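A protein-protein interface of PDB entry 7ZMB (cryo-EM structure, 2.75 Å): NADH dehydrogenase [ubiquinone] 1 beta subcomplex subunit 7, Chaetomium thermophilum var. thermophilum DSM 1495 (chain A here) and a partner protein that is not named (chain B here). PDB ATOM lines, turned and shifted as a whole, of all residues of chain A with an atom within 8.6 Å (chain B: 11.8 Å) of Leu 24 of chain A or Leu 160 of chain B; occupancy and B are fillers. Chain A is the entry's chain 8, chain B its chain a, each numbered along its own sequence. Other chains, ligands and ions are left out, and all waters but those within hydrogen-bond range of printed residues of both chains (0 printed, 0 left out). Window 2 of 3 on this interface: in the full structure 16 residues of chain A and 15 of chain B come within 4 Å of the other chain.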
ATOM      1  N   MET A  17     -12.217  23.924 -19.040  1.00  0.00           N
ATOM      2  CA  MET A  17     -13.650  23.997 -19.302  1.00  0.00           C
ATOM      3  C   MET A  17     -14.458  23.247 -18.252  1.00  0.00           C
ATOM      4  O   MET A  17     -15.606  23.618 -17.980  1.00  0.00           O
ATOM      5  CB  MET A  17     -13.930  23.480 -20.717  1.00  0.00           C
ATOM      6  CG  MET A  17     -15.372  23.538 -21.194  1.00  0.00           C
ATOM      7  SD  MET A  17     -16.370  22.155 -20.628  1.00  0.00           S
ATOM      8  CE  MET A  17     -15.699  20.843 -21.644  1.00  0.00           C
ATOM      9  N   ARG A  18     -13.883  22.208 -17.642  1.00  0.00           N
ATOM     10  CA  ARG A  18     -14.570  21.527 -16.549  1.00  0.00           C
ATOM     11  C   ARG A  18     -14.747  22.448 -15.349  1.00  0.00           C
ATOM     12  O   ARG A  18     -15.795  22.427 -14.693  1.00  0.00           O
ATOM     13  CB  ARG A  18     -13.804  20.266 -16.148  1.00  0.00           C
ATOM     14  CG  ARG A  18     -14.458  19.467 -15.032  1.00  0.00           C
ATOM     15  CD  ARG A  18     -13.706  19.621 -13.718  1.00  0.00           C
ATOM     16  NE  ARG A  18     -12.266  19.445 -13.881  1.00  0.00           N
ATOM     17  CZ  ARG A  18     -11.666  18.268 -14.025  1.00  0.00           C
ATOM     18  NH1 ARG A  18     -10.348  18.208 -14.166  1.00  0.00           N
ATOM     19  NH2 ARG A  18     -12.378  17.151 -14.031  1.00  0.00           N
ATOM     20  N   LYS A  21     -17.823  24.562 -15.078  1.00  0.00           N
ATOM     21  CA  LYS A  21     -19.039  23.901 -14.605  1.00  0.00           C
ATOM     22  C   LYS A  21     -20.214  24.197 -15.546  1.00  0.00           C
ATOM     23  O   LYS A  21     -21.186  24.873 -15.203  1.00  0.00           O
ATOM     24  CB  LYS A  21     -19.348  24.309 -13.157  1.00  0.00           C
ATOM     25  CG  LYS A  21     -20.517  23.574 -12.521  1.00  0.00           C
ATOM     26  CD  LYS A  21     -20.792  24.086 -11.118  1.00  0.00           C
ATOM     27  CE  LYS A  21     -19.736  23.612 -10.136  1.00  0.00           C
ATOM     28  NZ  LYS A  21     -20.065  24.014  -8.742  1.00  0.00           N
ATOM     29  N   VAL A  22     -20.074  23.687 -16.765  1.00  0.00           N
ATOM     30  CA  VAL A  22     -21.092  23.853 -17.797  1.00  0.00           C
ATOM     31  C   VAL A  22     -21.830  22.529 -17.967  1.00  0.00           C
ATOM     32  O   VAL A  22     -21.277  21.471 -17.635  1.00  0.00           O
ATOM     33  CB  VAL A  22     -20.466  24.332 -19.117  1.00  0.00           C
ATOM     34  CG1 VAL A  22     -19.671  25.603 -18.884  1.00  0.00           C
ATOM     35  CG2 VAL A  22     -19.593  23.252 -19.710  1.00  0.00           C
ATOM     36  N   PRO A  23     -23.068  22.533 -18.463  1.00  0.00           N
ATOM     37  CA  PRO A  23     -23.839  21.286 -18.541  1.00  0.00           C
ATOM     38  C   PRO A  23     -23.202  20.270 -19.479  1.00  0.00           C
ATOM     39  O   PRO A  23     -22.424  20.606 -20.374  1.00  0.00           O
ATOM     40  CB  PRO A  23     -25.204  21.744 -19.067  1.00  0.00           C
ATOM     41  CG  PRO A  23     -25.281  23.187 -18.710  1.00  0.00           C
ATOM     42  CD  PRO A  23     -23.884  23.705 -18.824  1.00  0.00           C
ATOM     43  N   LEU A  24     -23.550  19.000 -19.251  1.00  0.00           N
ATOM     44  CA  LEU A  24     -22.971  17.915 -20.037  1.00  0.00           C
ATOM     45  C   LEU A  24     -23.326  18.044 -21.512  1.00  0.00           C
ATOM     46  O   LEU A  24     -22.478  17.822 -22.385  1.00  0.00           O
ATOM     47  CB  LEU A  24     -23.439  16.557 -19.511  1.00  0.00           C
ATOM     48  CG  LEU A  24     -22.736  15.918 -18.312  1.00  0.00           C
ATOM     49  CD1 LEU A  24     -21.257  15.695 -18.600  1.00  0.00           C
ATOM     50  CD2 LEU A  24     -22.939  16.714 -17.044  1.00  0.00           C
ATOM     51  N   ALA A  25     -24.577  18.395 -21.813  1.00  0.00           N
ATOM     52  CA  ALA A  25     -25.019  18.476 -23.198  1.00  0.00           C
ATOM     53  C   ALA A  25     -24.347  19.600 -23.971  1.00  0.00           C
ATOM     54  O   ALA A  25     -24.472  19.644 -25.200  1.00  0.00           O
ATOM     55  CB  ALA A  25     -26.536  18.648 -23.255  1.00  0.00           C
ATOM     56  N   TYR A  26     -23.645  20.505 -23.292  1.00  0.00           N
ATOM     57  CA  TYR A  26     -22.989  21.636 -23.934  1.00  0.00           C
ATOM     58  C   TYR A  26     -21.479  21.597 -23.729  1.00  0.00           C
ATOM     59  O   TYR A  26     -20.811  22.631 -23.785  1.00  0.00           O
ATOM     60  CB  TYR A  26     -23.572  22.951 -23.421  1.00  0.00           C
ATOM     61  CG  TYR A  26     -25.074  23.031 -23.561  1.00  0.00           C
ATOM     62  CD1 TYR A  26     -25.709  22.557 -24.699  1.00  0.00           C
ATOM     63  CD2 TYR A  26     -25.857  23.567 -22.550  1.00  0.00           C
ATOM     64  CE1 TYR A  26     -27.080  22.622 -24.832  1.00  0.00           C
ATOM     65  CE2 TYR A  26     -27.230  23.637 -22.675  1.00  0.00           C
ATOM     66  CZ  TYR A  26     -27.835  23.163 -23.816  1.00  0.00           C
ATOM     67  OH  TYR A  26     -29.202  23.230 -23.944  1.00  0.00           O
ATOM     68  N   ARG A  27     -20.926  20.409 -23.491  1.00  0.00           N
ATOM     69  CA  ARG A  27     -19.483  20.228 -23.404  1.00  0.00           C
ATOM     70  C   ARG A  27     -18.801  20.222 -24.764  1.00  0.00           C
ATOM     71  O   ARG A  27     -17.613  19.893 -24.839  1.00  0.00           O
ATOM     72  CB  ARG A  27     -19.148  18.926 -22.671  1.00  0.00           C
ATOM     73  CG  ARG A  27     -19.642  18.836 -21.241  1.00  0.00           C
ATOM     74  CD  ARG A  27     -18.887  19.811 -20.369  1.00  0.00           C
ATOM     75  NE  ARG A  27     -19.315  19.785 -18.976  1.00  0.00           N
ATOM     76  CZ  ARG A  27     -18.775  18.994 -18.055  1.00  0.00           C
ATOM     77  NH1 ARG A  27     -17.790  18.171 -18.384  1.00  0.00           N
ATOM     78  NH2 ARG A  27     -19.214  19.026 -16.807  1.00  0.00           N
ATOM     79  N   ASP A  28     -19.514  20.572 -25.832  1.00  0.00           N
ATOM     80  CA  ASP A  28     -18.951  20.500 -27.168  1.00  0.00           C
ATOM     81  C   ASP A  28     -17.820  21.514 -27.336  1.00  0.00           C
ATOM     82  O   ASP A  28     -17.595  22.391 -26.498  1.00  0.00           O
ATOM     83  CB  ASP A  28     -20.036  20.734 -28.221  1.00  0.00           C
ATOM     84  CG  ASP A  28     -20.717  22.082 -28.073  1.00  0.00           C
ATOM     85  OD1 ASP A  28     -20.415  22.810 -27.105  1.00  0.00           O
ATOM     86  OD2 ASP A  28     -21.557  22.417 -28.936  1.00  0.00           O
ATOM     87  N   ALA A  31     -18.352  25.484 -27.090  1.00  0.00           N
ATOM     88  CA  ALA A  31     -18.715  26.109 -25.826  1.00  0.00           C
ATOM     89  C   ALA A  31     -17.709  27.153 -25.358  1.00  0.00           C
ATOM     90  O   ALA A  31     -17.851  27.660 -24.240  1.00  0.00           O
ATOM     91  CB  ALA A  31     -18.880  25.041 -24.744  1.00  0.00           C
ATOM     92  N   ARG B 150     -24.813  15.085 -32.373  1.00  0.00           N
ATOM     93  CA  ARG B 150     -23.724  15.982 -32.019  1.00  0.00           C
ATOM     94  C   ARG B 150     -22.427  15.206 -31.838  1.00  0.00           C
ATOM     95  O   ARG B 150     -22.412  14.109 -31.275  1.00  0.00           O
ATOM     96  CB  ARG B 150     -24.061  16.751 -30.743  1.00  0.00           C
ATOM     97  CG  ARG B 150     -25.481  17.287 -30.702  1.00  0.00           C
ATOM     98  CD  ARG B 150     -25.648  18.295 -29.582  1.00  0.00           C
ATOM     99  NE  ARG B 150     -25.058  19.586 -29.923  1.00  0.00           N
ATOM    100  CZ  ARG B 150     -24.101  20.179 -29.219  1.00  0.00           C
ATOM    101  NH1 ARG B 150     -23.624  21.354 -29.604  1.00  0.00           N
ATOM    102  NH2 ARG B 150     -23.619  19.596 -28.132  1.00  0.00           N
ATOM    103  N   GLU B 151     -21.337  15.781 -32.333  1.00  0.00           N
ATOM    104  CA  GLU B 151     -20.014  15.188 -32.205  1.00  0.00           C
ATOM    105  C   GLU B 151     -19.315  15.820 -31.010  1.00  0.00           C
ATOM    106  O   GLU B 151     -19.135  17.042 -30.964  1.00  0.00           O
ATOM    107  CB  GLU B 151     -19.198  15.388 -33.480  1.00  0.00           C
ATOM    108  CG  GLU B 151     -17.839  14.707 -33.459  1.00  0.00           C
ATOM    109  CD  GLU B 151     -17.940  13.198 -33.554  1.00  0.00           C
ATOM    110  OE1 GLU B 151     -18.978  12.698 -34.035  1.00  0.00           O
ATOM    111  OE2 GLU B 151     -16.979  12.510 -33.147  1.00  0.00           O
ATOM    112  N   PHE B 152     -18.928  14.991 -30.049  1.00  0.00           N
ATOM    113  CA  PHE B 152     -18.248  15.439 -28.843  1.00  0.00           C
ATOM    114  C   PHE B 152     -16.810  14.951 -28.874  1.00  0.00           C
ATOM    115  O   PHE B 152     -16.563  13.751 -29.030  1.00  0.00           O
ATOM    116  CB  PHE B 152     -18.956  14.916 -27.595  1.00  0.00           C
ATOM    117  CG  PHE B 152     -20.266  15.588 -27.313  1.00  0.00           C
ATOM    118  CD1 PHE B 152     -20.309  16.810 -26.667  1.00  0.00           C
ATOM    119  CD2 PHE B 152     -21.458  14.992 -27.689  1.00  0.00           C
ATOM    120  CE1 PHE B 152     -21.513  17.427 -26.404  1.00  0.00           C
ATOM    121  CE2 PHE B 152     -22.666  15.605 -27.429  1.00  0.00           C
ATOM    122  CZ  PHE B 152     -22.694  16.823 -26.786  1.00  0.00           C
ATOM    123  N   GLU B 153     -15.868  15.876 -28.723  1.00  0.00           N
ATOM    124  CA  GLU B 153     -14.457  15.516 -28.771  1.00  0.00           C
ATOM    125  C   GLU B 153     -14.100  14.668 -27.555  1.00  0.00           C
ATOM    126  O   GLU B 153     -14.444  15.015 -26.420  1.00  0.00           O
ATOM    127  CB  GLU B 153     -13.591  16.772 -28.858  1.00  0.00           C
ATOM    128  CG  GLU B 153     -13.783  17.785 -27.738  1.00  0.00           C
ATOM    129  CD  GLU B 153     -12.902  17.512 -26.538  1.00  0.00           C
ATOM    130  OE1 GLU B 153     -11.890  16.797 -26.693  1.00  0.00           O
ATOM    131  OE2 GLU B 153     -13.221  18.016 -25.441  1.00  0.00           O
ATOM    132  N   GLY B 154     -13.447  13.535 -27.801  1.00  0.00           N
ATOM    133  CA  GLY B 154     -13.105  12.600 -26.752  1.00  0.00           C
ATOM    134  C   GLY B 154     -14.230  11.692 -26.311  1.00  0.00           C
ATOM    135  O   GLY B 154     -13.980  10.749 -25.552  1.00  0.00           O
ATOM    136  N   GLY B 155     -15.458  11.941 -26.761  1.00  0.00           N
ATOM    137  CA  GLY B 155     -16.586  11.101 -26.425  1.00  0.00           C
ATOM    138  C   GLY B 155     -17.154  11.298 -25.037  1.00  0.00           C
ATOM    139  O   GLY B 155     -18.073  10.562 -24.659  1.00  0.00           O
ATOM    140  N   LEU B 156     -16.647  12.266 -24.271  1.00  0.00           N
ATOM    141  CA  LEU B 156     -17.090  12.500 -22.894  1.00  0.00           C
ATOM    142  C   LEU B 156     -16.978  11.230 -22.055  1.00  0.00           C
ATOM    143  O   LEU B 156     -17.847  10.927 -21.235  1.00  0.00           O
ATOM    144  CB  LEU B 156     -18.515  13.059 -22.852  1.00  0.00           C
ATOM    145  CG  LEU B 156     -18.706  14.576 -22.952  1.00  0.00           C
ATOM    146  CD1 LEU B 156     -18.113  15.268 -21.742  1.00  0.00           C
ATOM    147  CD2 LEU B 156     -18.091  15.133 -24.215  1.00  0.00           C
ATOM    148  N   GLU B 157     -15.897  10.479 -22.266  1.00  0.00           N
ATOM    149  CA  GLU B 157     -15.689   9.246 -21.514  1.00  0.00           C
ATOM    150  C   GLU B 157     -15.499   9.530 -20.031  1.00  0.00           C
ATOM    151  O   GLU B 157     -16.167   8.930 -19.180  1.00  0.00           O
ATOM    152  CB  GLU B 157     -14.483   8.491 -22.073  1.00  0.00           C
ATOM    153  CG  GLU B 157     -14.777   7.673 -23.315  1.00  0.00           C
ATOM    154  CD  GLU B 157     -15.477   6.367 -22.994  1.00  0.00           C
ATOM    155  OE1 GLU B 157     -15.171   5.773 -21.940  1.00  0.00           O
ATOM    156  OE2 GLU B 157     -16.333   5.938 -23.793  1.00  0.00           O
ATOM    157  N   ARG B 158     -14.593  10.451 -19.702  1.00  0.00           N
ATOM    158  CA  ARG B 158     -14.279  10.715 -18.302  1.00  0.00           C
ATOM    159  C   ARG B 158     -15.448  11.377 -17.585  1.00  0.00           C
ATOM    160  O   ARG B 158     -15.846  10.947 -16.497  1.00  0.00           O
ATOM    161  CB  ARG B 158     -13.027  11.587 -18.205  1.00  0.00           C
ATOM    162  CG  ARG B 158     -12.360  11.561 -16.843  1.00  0.00           C
ATOM    163  CD  ARG B 158     -11.200  12.539 -16.780  1.00  0.00           C
ATOM    164  NE  ARG B 158     -10.296  12.388 -17.916  1.00  0.00           N
ATOM    165  CZ  ARG B 158      -9.973  13.372 -18.747  1.00  0.00           C
ATOM    166  NH1 ARG B 158      -9.143  13.146 -19.757  1.00  0.00           N
ATOM    167  NH2 ARG B 158     -10.478  14.586 -18.568  1.00  0.00           N
ATOM    168  N   GLU B 159     -16.020  12.420 -18.188  1.00  0.00           N
ATOM    169  CA  GLU B 159     -17.010  13.240 -17.500  1.00  0.00           C
ATOM    170  C   GLU B 159     -18.319  12.505 -17.246  1.00  0.00           C
ATOM    171  O   GLU B 159     -19.073  12.905 -16.353  1.00  0.00           O
ATOM    172  CB  GLU B 159     -17.280  14.513 -18.300  1.00  0.00           C
ATOM    173  CG  GLU B 159     -16.043  15.361 -18.569  1.00  0.00           C
ATOM    174  CD  GLU B 159     -15.254  14.886 -19.774  1.00  0.00           C
ATOM    175  OE1 GLU B 159     -15.598  13.824 -20.335  1.00  0.00           O
ATOM    176  OE2 GLU B 159     -14.290  15.578 -20.165  1.00  0.00           O
ATOM    177  N   LEU B 160     -18.608  11.445 -17.997  1.00  0.00           N
ATOM    178  CA  LEU B 160     -19.861  10.718 -17.855  1.00  0.00           C
ATOM    179  C   LEU B 160     -19.724   9.459 -17.012  1.00  0.00           C
ATOM    180  O   LEU B 160     -20.548   8.550 -17.143  1.00  0.00           O
ATOM    181  CB  LEU B 160     -20.428  10.367 -19.229  1.00  0.00           C
ATOM    182  CG  LEU B 160     -20.959  11.557 -20.024  1.00  0.00           C
ATOM    183  CD1 LEU B 160     -21.432  11.119 -21.399  1.00  0.00           C
ATOM    184  CD2 LEU B 160     -22.069  12.234 -19.259  1.00  0.00           C
ATOM    185  N   GLY B 161     -18.711   9.382 -16.156  1.00  0.00           N
ATOM    186  CA  GLY B 161     -18.552   8.256 -15.262  1.00  0.00           C
ATOM    187  C   GLY B 161     -17.572   7.192 -15.700  1.00  0.00           C
ATOM    188  O   GLY B 161     -17.565   6.107 -15.109  1.00  0.00           O
ATOM    189  N   GLY B 162     -16.754   7.459 -16.708  1.00  0.00           N
ATOM    190  CA  GLY B 162     -15.769   6.493 -17.150  1.00  0.00           C
ATOM    191  C   GLY B 162     -16.304   5.528 -18.186  1.00  0.00           C
ATOM    192  O   GLY B 162     -17.431   5.635 -18.682  1.00  0.00           O
ATOM    193  N   ALA B 163     -15.454   4.553 -18.518  1.00  0.00           N
ATOM    194  CA  ALA B 163     -15.809   3.569 -19.536  1.00  0.00           C
ATOM    195  C   ALA B 163     -17.005   2.727 -19.116  1.00  0.00           C
ATOM    196  O   ALA B 163     -17.757   2.247 -19.971  1.00  0.00           O
ATOM    197  CB  ALA B 163     -14.611   2.671 -19.839  1.00  0.00           C
ATOM    198  N   GLY B 164     -17.199   2.535 -17.815  1.00  0.00           N
ATOM    199  CA  GLY B 164     -18.320   1.757 -17.329  1.00  0.00           C
ATOM    200  C   GLY B 164     -19.603   2.556 -17.249  1.00  0.00           C
ATOM    201  O   GLY B 164     -20.283   2.549 -16.219  1.00  0.00           O
ATOM    202  N   ALA B 165     -19.942   3.252 -18.330  1.00  0.00           N
ATOM    203  CA  ALA B 165     -21.144   4.073 -18.371  1.00  0.00           C
ATOM    204  C   ALA B 165     -21.488   4.353 -19.827  1.00  0.00           C
ATOM    205  O   ALA B 165     -20.705   4.075 -20.736  1.00  0.00           O
ATOM    206  CB  ALA B 165     -20.960   5.377 -17.593  1.00  0.00           C
ATOM    207  N   VAL B 166     -22.681   4.908 -20.034  1.00  0.00           N
ATOM    208  CA  VAL B 166     -23.101   5.290 -21.375  1.00  0.00           C
ATOM    209  C   VAL B 166     -22.300   6.505 -21.823  1.00  0.00           C
ATOM    210  O   VAL B 166     -22.163   7.491 -21.087  1.00  0.00           O
ATOM    211  CB  VAL B 166     -24.613   5.554 -21.413  1.00  0.00           C
ATOM    212  CG1 VAL B 166     -25.011   6.597 -20.374  1.00  0.00           C
ATOM    213  CG2 VAL B 166     -25.041   5.989 -22.806  1.00  0.00           C
ATOM    214  N   ARG B 167     -21.749   6.433 -23.030  1.00  0.00           N
ATOM    215  CA  ARG B 167     -20.890   7.474 -23.571  1.00  0.00           C
ATOM    216  C   ARG B 167     -21.641   8.288 -24.617  1.00  0.00           C
ATOM    217  O   ARG B 167     -22.765   7.965 -25.008  1.00  0.00           O
ATOM    218  CB  ARG B 167     -19.622   6.867 -24.179  1.00  0.00           C
ATOM    219  CG  ARG B 167     -19.851   6.163 -25.504  1.00  0.00           C
ATOM    220  CD  ARG B 167     -18.669   5.289 -25.878  1.00  0.00           C
ATOM    221  NE  ARG B 167     -17.548   6.076 -26.382  1.00  0.00           N
ATOM    222  CZ  ARG B 167     -17.398   6.432 -27.653  1.00  0.00           C
ATOM    223  NH1 ARG B 167     -18.301   6.071 -28.553  1.00  0.00           N
ATOM    224  NH2 ARG B 167     -16.347   7.147 -28.024  1.00  0.00           N
ATOM    225  N   ALA B 168     -20.997   9.359 -25.067  1.00  0.00           N
ATOM    226  CA  ALA B 168     -21.562  10.231 -26.083  1.00  0.00           C
ATOM    227  C   ALA B 168     -21.252   9.668 -27.469  1.00  0.00           C
ATOM    228  O   ALA B 168     -20.726   8.563 -27.614  1.00  0.00           O
ATOM    229  CB  ALA B 168     -21.034  11.652 -25.913  1.00  0.00           C
ATOM    230  N   PHE B 169     -21.577  10.433 -28.508  1.00  0.00           N
ATOM    231  CA  PHE B 169     -21.334  10.019 -29.880  1.00  0.00           C
ATOM    232  C   PHE B 169     -19.968  10.524 -30.325  1.00  0.00           C
ATOM    233  O   PHE B 169     -19.683  11.722 -30.233  1.00  0.00           O
ATOM    234  CB  PHE B 169     -22.428  10.555 -30.804  1.00  0.00           C
ATOM    235  CG  PHE B 169     -22.274  10.135 -32.235  1.00  0.00           C
ATOM    236  CD1 PHE B 169     -22.596   8.849 -32.632  1.00  0.00           C
ATOM    237  CD2 PHE B 169     -21.800  11.024 -33.184  1.00  0.00           C
ATOM    238  CE1 PHE B 169     -22.455   8.459 -33.950  1.00  0.00           C
ATOM    239  CE2 PHE B 169     -21.653  10.638 -34.502  1.00  0.00           C
ATOM    240  CZ  PHE B 169     -21.981   9.354 -34.885  1.00  0.00           C
ATOM    241  N   LEU B 170     -19.123   9.608 -30.805  1.00  0.00           N
ATOM    242  CA  LEU B 170     -17.769   9.972 -31.228  1.00  0.00           C
ATOM    243  C   LEU B 170     -17.368   9.051 -32.384  1.00  0.00           C
ATOM    244  O   LEU B 170     -16.887   7.936 -32.168  1.00  0.00           O
ATOM    245  CB  LEU B 170     -16.785   9.885 -30.071  1.00  0.00           C
ATOM    246  CG  LEU B 170     -15.302  10.059 -30.409  1.00  0.00           C
ATOM    247  CD1 LEU B 170     -14.990  11.507 -30.741  1.00  0.00           C
ATOM    248  CD2 LEU B 170     -14.431   9.572 -29.261  1.00  0.00           C
ATOM    249  N   LEU B 172     -18.900   7.223 -34.484  1.00  0.00           N
ATOM    250  CA  LEU B 172     -19.529   5.914 -34.510  1.00  0.00           C
ATOM    251  C   LEU B 172     -20.362   5.766 -35.781  1.00  0.00           C
ATOM    252  O   LEU B 172     -20.336   6.618 -36.673  1.00  0.00           O
ATOM    253  CB  LEU B 172     -20.381   5.711 -33.256  1.00  0.00           C
ATOM    254  CG  LEU B 172     -19.703   5.918 -31.901  1.00  0.00           C
ATOM    255  CD1 LEU B 172     -20.733   5.843 -30.785  1.00  0.00           C
ATOM    256  CD2 LEU B 172     -18.600   4.895 -31.687  1.00  0.00           C
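N of Phe 152 of chain B is in hydrogen-bond range of O of Phe 169 of chain B, 3.4 Å away. NE of Arg 27 of chain A sits at hydrogen-bond distance from O of Val 22 of chain A (2.9 Å). The backbone NH of Ala 31 of chain A lies within hydrogen-bond range of the side-chain carboxylate of Asp 28 of chain A, at 3.4 Å.
The backbone carbonyl oxygen (O) of Ala 25 of chain A sits at hydrogen-bond distance from the guanidinium group (NH2) of Arg 150 of chain B (3.1 Å). NH1 of Arg 150 of chain B is in salt-bridge range of OD2 of Asp 28 of chain A (2.4 Å).
Leu 160 of chain B touches Leu 24 of chain A. Ala 25 of chain A touches Phe 152 of chain B. Arg 27 of chain A touches Leu 156 of chain B. Arg 27 of chain A touches Glu 159 of chain B (NH1 to CG, 3.3 Å). Asp 28 of chain A touches Phe 152 of chain B.
Of the 22 printed residues of chain B, 5 touch a printed residue of chain A. Hydrophobic or aromatic side chains of chain B that line the printed part of chain A: Phe 152, Leu 156 and Leu 160. Printed residues of chain A that touch a printed residue of chain B: Leu 24, Ala 25, Arg 27 and Asp 28. Hydrophobic or aromatic side chains of chain A within 4 Å of the printed part of chain B: Leu 24. Among the printed residues, Asp or Glu carboxylates within 4 Å of a Lys or Arg side-chain nitrogen of the other chain: Asp 28 of chain A with Arg 150 of chain B (2.4 Å).
Leu 24 of chain A touches just one residue of chain B: Leu 160 (3.6 Å). Leu 160 of chain B touches just one residue of chain A: Leu 24 (3.6 Å). No residue of chain B comes within 4 Å of Val 22 of chain A. Printed residues of chain B within 4 Å of Asp 28 of chain A: Arg 150 and Phe 152. Printed residues of chain A within 4 Å of Arg 150 of chain B: Ala 25 (3.1 Å) and Asp 28 (2.4 Å). Printed residues of chain A within 4 Å of Phe 152 of chain B: Ala 25 (3.7 Å) and Asp 28 (3.8 Å). Of the printed residues of chain A, Leu 156 of chain B touches Arg 27 (3.9 Å). Printed residues of chain A within 4 Å of Glu 159 of chain B: Arg 27 (3.3 Å). Val 166 of chain B touches none of the printed residues of chain A. Ala 165 of chain B touches none of the printed residues of chain A. The nearest printed residue of chain B that does not touch Leu 24 of chain A is Phe 152 of chain B (4.2 Å). The nearest printed residue of chain B that does not touch Asp 28 of chain A is Glu 151 of chain B (4.7 Å).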
